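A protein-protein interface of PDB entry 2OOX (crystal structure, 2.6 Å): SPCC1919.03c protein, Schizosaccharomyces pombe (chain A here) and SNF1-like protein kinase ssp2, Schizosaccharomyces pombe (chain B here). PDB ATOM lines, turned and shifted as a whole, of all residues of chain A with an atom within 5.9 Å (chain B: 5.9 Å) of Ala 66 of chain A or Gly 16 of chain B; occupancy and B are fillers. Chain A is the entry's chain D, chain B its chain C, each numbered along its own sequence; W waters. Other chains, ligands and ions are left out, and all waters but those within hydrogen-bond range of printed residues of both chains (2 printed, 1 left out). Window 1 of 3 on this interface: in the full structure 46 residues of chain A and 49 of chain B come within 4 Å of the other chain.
O of His 14 of chain B is in hydrogen-bond range of N of Ala 66 of chain A. The backbone NH (N) of Gly 16 of chain B is in hydrogen-bond range of the backbone carbonyl oxygen (O) of Leu 64 of chain A (3.0 Å). O of Val 94 of chain B lies within hydrogen-bond range of N of Leu 64 of chain A.
ND1 of His 14 of chain B sits close to O of Gly 16 of chain B (3.4 Å). The guanidinium group of Arg 18 of chain B sits at hydrogen-bond distance from a ring nitrogen (NE2) of His 14 of chain B, 3.2 Å away. The backbone NH (N) of Ser 77 of chain A sits at hydrogen-bond distance from the backbone carbonyl oxygen (O) of Ala 65 of chain A, at 2.9 Å. O of Ala 75 of chain A lies within hydrogen-bond range of N of Ala 67 of chain A (3.1 Å).
Among the printed residues, pairs that only touch across the chains: Leu 64 of chain A with Phe 15 of chain B, Ala 65 of chain A with Trp 13 of chain B, Ala 65 of chain A with His 14 of chain B, Ala 66 of chain A with Trp 13 of chain B, Ala 66 of chain A with Gly 16 of chain B, Ala 67 of chain A with Lys 12 of chain B, Ala 67 of chain A with Trp 13 of chain B, Ala 75 of chain A with Trp 13 of chain B, Leu 76 of chain A with Trp 13 of chain B and Ser 77 of chain A with Trp 13 of chain B.
Ala 66 of chain A touches three residues of chain B. Printed residues of chain A within 4 Å of Phe 15 of chain B: Leu 64. Printed residues of chain A within 4 Å of Trp 13 of chain B: Ala 65, Ala 66, Ala 67, Ala 75, Leu 76 and Ser 77. Of the printed residues of chain A, Val 94 of chain B touches Leu 64 (2.8 Å). Arg 18 of chain B touches none of the printed residues of chain A. Val 17 of chain B touches none of the printed residues of chain A. The nearest residue of chain B that does not touch Ala 66 of chain A is Lys 12 of chain B (4.05 Å). The nearest residue of chain A that does not touch Gly 16 of chain B is Ala 65 of chain A (4.2 Å).
Printed residues of chain A that touch a printed residue of chain B: Leu 64, Ala 65, Ala 66, Ala 67, Ala 75, Leu 76 and Ser 77. Hydrophobic or aromatic side chains of chain B that line the printed part of chain A: Trp 13, His 14, Phe 15 and Val 94.
Water W2 lies within hydrogen-bond range of OD1 of Asp 93 of chain B (2.5 Å), O of Leu 64 of chain A (2.9 Å), N of Gly 16 of chain B (3.1 Å) and N of Val 94 of chain B (3.1 Å). Water W1 bridges the backbone carbonyl oxygen of Lys 12 of chain B and the backbone NH of Asn 68 of chain A.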
ATOM      1  N   LEU A  64      17.218  -4.963 -15.057  1.00  0.00           N
ATOM      2  CA  LEU A  64      16.654  -3.631 -15.232  1.00  0.00           C
ATOM      3  C   LEU A  64      17.607  -2.748 -16.001  1.00  0.00           C
ATOM      4  O   LEU A  64      18.806  -2.817 -15.795  1.00  0.00           O
ATOM      5  CB  LEU A  64      16.393  -3.015 -13.861  1.00  0.00           C
ATOM      6  CG  LEU A  64      16.065  -1.533 -13.891  1.00  0.00           C
ATOM      7  CD1 LEU A  64      14.694  -1.329 -14.561  1.00  0.00           C
ATOM      8  CD2 LEU A  64      16.118  -0.916 -12.496  1.00  0.00           C
ATOM      9  N   ALA A  65      17.059  -1.926 -16.890  1.00  0.00           N
ATOM     10  CA  ALA A  65      17.805  -0.936 -17.656  1.00  0.00           C
ATOM     11  C   ALA A  65      16.978   0.338 -17.636  1.00  0.00           C
ATOM     12  O   ALA A  65      15.757   0.274 -17.436  1.00  0.00           O
ATOM     13  CB  ALA A  65      18.027  -1.419 -19.059  1.00  0.00           C
ATOM     14  N   ALA A  66      17.621   1.490 -17.800  1.00  0.00           N
ATOM     15  CA  ALA A  66      16.988   2.774 -17.412  1.00  0.00           C
ATOM     16  C   ALA A  66      17.532   3.847 -18.327  1.00  0.00           C
ATOM     17  O   ALA A  66      18.645   3.683 -18.874  1.00  0.00           O
ATOM     18  CB  ALA A  66      17.270   3.113 -15.913  1.00  0.00           C
ATOM     19  N   ALA A  67      16.749   4.901 -18.566  1.00  0.00           N
ATOM     20  CA  ALA A  67      17.268   6.078 -19.305  1.00  0.00           C
ATOM     21  C   ALA A  67      16.517   7.318 -18.918  1.00  0.00           C
ATOM     22  O   ALA A  67      15.369   7.236 -18.490  1.00  0.00           O
ATOM     23  CB  ALA A  67      17.193   5.880 -20.804  1.00  0.00           C
ATOM     24  N   ASN A  68      17.198   8.456 -19.031  1.00  0.00           N
ATOM     25  CA  ASN A  68      16.602   9.786 -18.838  1.00  0.00           C
ATOM     26  C   ASN A  68      15.628  10.124 -19.947  1.00  0.00           C
ATOM     27  O   ASN A  68      15.956   9.985 -21.126  1.00  0.00           O
ATOM     28  CB  ASN A  68      17.704  10.846 -18.872  1.00  0.00           C
ATOM     29  CG  ASN A  68      18.621  10.792 -17.656  1.00  0.00           C
ATOM     30  OD1 ASN A  68      18.251  10.231 -16.607  1.00  0.00           O
ATOM     31  ND2 ASN A  68      19.827  11.381 -17.784  1.00  0.00           N
ATOM     32  N   ALA A  75      11.736   5.585 -17.715  1.00  0.00           N
ATOM     33  CA  ALA A  75      12.002   4.758 -18.859  1.00  0.00           C
ATOM     34  C   ALA A  75      12.779   3.534 -18.341  1.00  0.00           C
ATOM     35  O   ALA A  75      13.936   3.636 -17.953  1.00  0.00           O
ATOM     36  CB  ALA A  75      12.789   5.529 -19.876  1.00  0.00           C
ATOM     37  N   LEU A  76      12.131   2.375 -18.381  1.00  0.00           N
ATOM     38  CA  LEU A  76      12.571   1.159 -17.723  1.00  0.00           C
ATOM     39  C   LEU A  76      12.436   0.026 -18.719  1.00  0.00           C
ATOM     40  O   LEU A  76      11.395  -0.111 -19.382  1.00  0.00           O
ATOM     41  CB  LEU A  76      11.678   0.878 -16.518  1.00  0.00           C
ATOM     42  CG  LEU A  76      11.778   1.950 -15.437  1.00  0.00           C
ATOM     43  CD1 LEU A  76      10.921   1.720 -14.249  1.00  0.00           C
ATOM     44  CD2 LEU A  76      13.216   2.122 -14.990  1.00  0.00           C
ATOM     45  N   SER A  77      13.473  -0.799 -18.847  1.00  0.00           N
ATOM     46  CA  SER A  77      13.358  -1.919 -19.767  1.00  0.00           C
ATOM     47  C   SER A  77      13.937  -3.192 -19.167  1.00  0.00           C
ATOM     48  O   SER A  77      14.504  -3.174 -18.063  1.00  0.00           O
ATOM     49  CB  SER A  77      14.003  -1.601 -21.126  1.00  0.00           C
ATOM     50  OG  SER A  77      15.409  -1.432 -20.978  1.00  0.00           O
ATOM     51  N   LYS B  12      20.876   7.336 -24.122  1.00  0.00           N
ATOM     52  CA  LYS B  12      21.530   6.083 -23.816  1.00  0.00           C
ATOM     53  C   LYS B  12      20.866   5.364 -22.646  1.00  0.00           C
ATOM     54  O   LYS B  12      20.690   5.924 -21.554  1.00  0.00           O
ATOM     55  CB  LYS B  12      23.028   6.302 -23.567  1.00  0.00           C
ATOM     56  CG  LYS B  12      23.833   6.765 -24.790  1.00  0.00           C
ATOM     57  CD  LYS B  12      24.719   5.644 -25.339  1.00  0.00           C
ATOM     58  CE  LYS B  12      25.452   6.063 -26.620  1.00  0.00           C
ATOM     59  NZ  LYS B  12      25.562   4.902 -27.556  1.00  0.00           N
ATOM     60  N   TRP B  13      20.484   4.117 -22.898  1.00  0.00           N
ATOM     61  CA  TRP B  13      20.052   3.239 -21.830  1.00  0.00           C
ATOM     62  C   TRP B  13      21.291   2.735 -21.121  1.00  0.00           C
ATOM     63  O   TRP B  13      22.378   2.686 -21.688  1.00  0.00           O
ATOM     64  CB  TRP B  13      19.261   2.073 -22.394  1.00  0.00           C
ATOM     65  CG  TRP B  13      17.958   2.481 -22.974  1.00  0.00           C
ATOM     66  CD1 TRP B  13      17.745   3.059 -24.201  1.00  0.00           C
ATOM     67  CD2 TRP B  13      16.663   2.334 -22.371  1.00  0.00           C
ATOM     68  NE1 TRP B  13      16.409   3.275 -24.391  1.00  0.00           N
ATOM     69  CE2 TRP B  13      15.717   2.849 -23.287  1.00  0.00           C
ATOM     70  CE3 TRP B  13      16.215   1.814 -21.160  1.00  0.00           C
ATOM     71  CZ2 TRP B  13      14.351   2.869 -23.022  1.00  0.00           C
ATOM     72  CZ3 TRP B  13      14.855   1.841 -20.897  1.00  0.00           C
ATOM     73  CH2 TRP B  13      13.937   2.361 -21.827  1.00  0.00           C
ATOM     74  N   HIS B  14      21.131   2.349 -19.874  1.00  0.00           N
ATOM     75  CA  HIS B  14      22.235   1.787 -19.144  1.00  0.00           C
ATOM     76  C   HIS B  14      21.606   0.870 -18.146  1.00  0.00           C
ATOM     77  O   HIS B  14      20.506   1.147 -17.669  1.00  0.00           O
ATOM     78  CB  HIS B  14      22.975   2.899 -18.417  1.00  0.00           C
ATOM     79  CG  HIS B  14      22.080   3.750 -17.580  1.00  0.00           C
ATOM     80  ND1 HIS B  14      21.808   3.461 -16.265  1.00  0.00           N
ATOM     81  CD2 HIS B  14      21.359   4.856 -17.883  1.00  0.00           C
ATOM     82  CE1 HIS B  14      20.982   4.374 -15.778  1.00  0.00           C
ATOM     83  NE2 HIS B  14      20.670   5.217 -16.749  1.00  0.00           N
ATOM     84  N   PHE B  15      22.302  -0.209 -17.807  1.00  0.00           N
ATOM     85  CA  PHE B  15      21.772  -1.126 -16.826  1.00  0.00           C
ATOM     86  C   PHE B  15      21.698  -0.445 -15.475  1.00  0.00           C
ATOM     87  O   PHE B  15      22.424   0.507 -15.201  1.00  0.00           O
ATOM     88  CB  PHE B  15      22.610  -2.389 -16.762  1.00  0.00           C
ATOM     89  CG  PHE B  15      22.484  -3.271 -17.975  1.00  0.00           C
ATOM     90  CD1 PHE B  15      23.513  -3.366 -18.883  1.00  0.00           C
ATOM     91  CD2 PHE B  15      21.341  -4.022 -18.195  1.00  0.00           C
ATOM     92  CE1 PHE B  15      23.408  -4.203 -20.004  1.00  0.00           C
ATOM     93  CE2 PHE B  15      21.225  -4.844 -19.328  1.00  0.00           C
ATOM     94  CZ  PHE B  15      22.248  -4.940 -20.221  1.00  0.00           C
ATOM     95  N   GLY B  16      20.780  -0.914 -14.649  1.00  0.00           N
ATOM     96  CA  GLY B  16      20.666  -0.452 -13.280  1.00  0.00           C
ATOM     97  C   GLY B  16      20.329   1.014 -13.155  1.00  0.00           C
ATOM     98  O   GLY B  16      19.901   1.645 -14.118  1.00  0.00           O
ATOM     99  N   VAL B  17      20.520   1.536 -11.957  1.00  0.00           N
ATOM    100  CA  VAL B  17      20.300   2.924 -11.638  1.00  0.00           C
ATOM    101  C   VAL B  17      21.637   3.536 -11.230  1.00  0.00           C
ATOM    102  O   VAL B  17      22.349   2.965 -10.381  1.00  0.00           O
ATOM    103  CB  VAL B  17      19.417   3.025 -10.386  1.00  0.00           C
ATOM    104  CG1 VAL B  17      19.273   4.455  -9.967  1.00  0.00           C
ATOM    105  CG2 VAL B  17      18.062   2.322 -10.576  1.00  0.00           C
ATOM    106  N   ARG B  18      21.964   4.701 -11.789  1.00  0.00           N
ATOM    107  CA  ARG B  18      23.210   5.385 -11.455  1.00  0.00           C
ATOM    108  C   ARG B  18      23.182   5.941 -10.048  1.00  0.00           C
ATOM    109  O   ARG B  18      22.188   6.478  -9.590  1.00  0.00           O
ATOM    110  CB  ARG B  18      23.488   6.519 -12.414  1.00  0.00           C
ATOM    111  CG  ARG B  18      23.875   6.105 -13.800  1.00  0.00           C
ATOM    112  CD  ARG B  18      24.519   7.312 -14.513  1.00  0.00           C
ATOM    113  NE  ARG B  18      24.626   7.146 -15.965  1.00  0.00           N
ATOM    114  CZ  ARG B  18      23.633   7.383 -16.824  1.00  0.00           C
ATOM    115  NH1 ARG B  18      22.452   7.799 -16.375  1.00  0.00           N
ATOM    116  NH2 ARG B  18      23.817   7.207 -18.133  1.00  0.00           N
ATOM    117  N   MET B  91      26.989   1.528 -10.113  1.00  0.00           N
ATOM    118  CA  MET B  91      25.753   1.027 -10.680  1.00  0.00           C
ATOM    119  C   MET B  91      25.024   0.158  -9.646  1.00  0.00           C
ATOM    120  O   MET B  91      25.630  -0.721  -9.000  1.00  0.00           O
ATOM    121  CB  MET B  91      26.019   0.210 -11.959  1.00  0.00           C
ATOM    122  CG  MET B  91      24.730  -0.357 -12.604  1.00  0.00           C
ATOM    123  SD  MET B  91      24.980  -1.700 -13.753  1.00  0.00           S
ATOM    124  CE  MET B  91      25.846  -0.876 -15.073  1.00  0.00           C
ATOM    125  N   LEU B  92      23.730   0.400  -9.498  1.00  0.00           N
ATOM    126  CA  LEU B  92      22.896  -0.458  -8.692  1.00  0.00           C
ATOM    127  C   LEU B  92      22.108  -1.343  -9.652  1.00  0.00           C
ATOM    128  O   LEU B  92      21.086  -0.941 -10.231  1.00  0.00           O
ATOM    129  CB  LEU B  92      21.963   0.349  -7.786  1.00  0.00           C
ATOM    130  CG  LEU B  92      20.913  -0.482  -7.033  1.00  0.00           C
ATOM    131  CD1 LEU B  92      21.561  -1.516  -6.078  1.00  0.00           C
ATOM    132  CD2 LEU B  92      19.898   0.389  -6.299  1.00  0.00           C
ATOM    133  N   ASP B  93      22.608  -2.553  -9.827  1.00  0.00           N
ATOM    134  CA  ASP B  93      22.104  -3.459 -10.817  1.00  0.00           C
ATOM    135  C   ASP B  93      20.964  -4.194 -10.165  1.00  0.00           C
ATOM    136  O   ASP B  93      21.101  -4.670  -9.039  1.00  0.00           O
ATOM    137  CB  ASP B  93      23.225  -4.405 -11.257  1.00  0.00           C
ATOM    138  CG  ASP B  93      22.704  -5.634 -11.931  1.00  0.00           C
ATOM    139  OD1 ASP B  93      22.455  -5.597 -13.146  1.00  0.00           O
ATOM    140  OD2 ASP B  93      22.529  -6.655 -11.242  1.00  0.00           O
ATOM    141  N   VAL B  94      19.842  -4.280 -10.876  1.00  0.00           N
ATOM    142  CA  VAL B  94      18.618  -4.881 -10.348  1.00  0.00           C
ATOM    143  C   VAL B  94      18.189  -5.974 -11.306  1.00  0.00           C
ATOM    144  O   VAL B  94      18.076  -5.753 -12.521  1.00  0.00           O
ATOM    145  CB  VAL B  94      17.488  -3.829 -10.227  1.00  0.00           C
ATOM    146  CG1 VAL B  94      16.369  -4.326  -9.313  1.00  0.00           C
ATOM    147  CG2 VAL B  94      18.035  -2.490  -9.703  1.00  0.00           C
HETATM  148  O   HOH W   1      20.112   7.780 -19.599  1.00  0.00           O
HETATM  149  O   HOH W   2      20.688  -3.919 -13.871  1.00  0.00           O
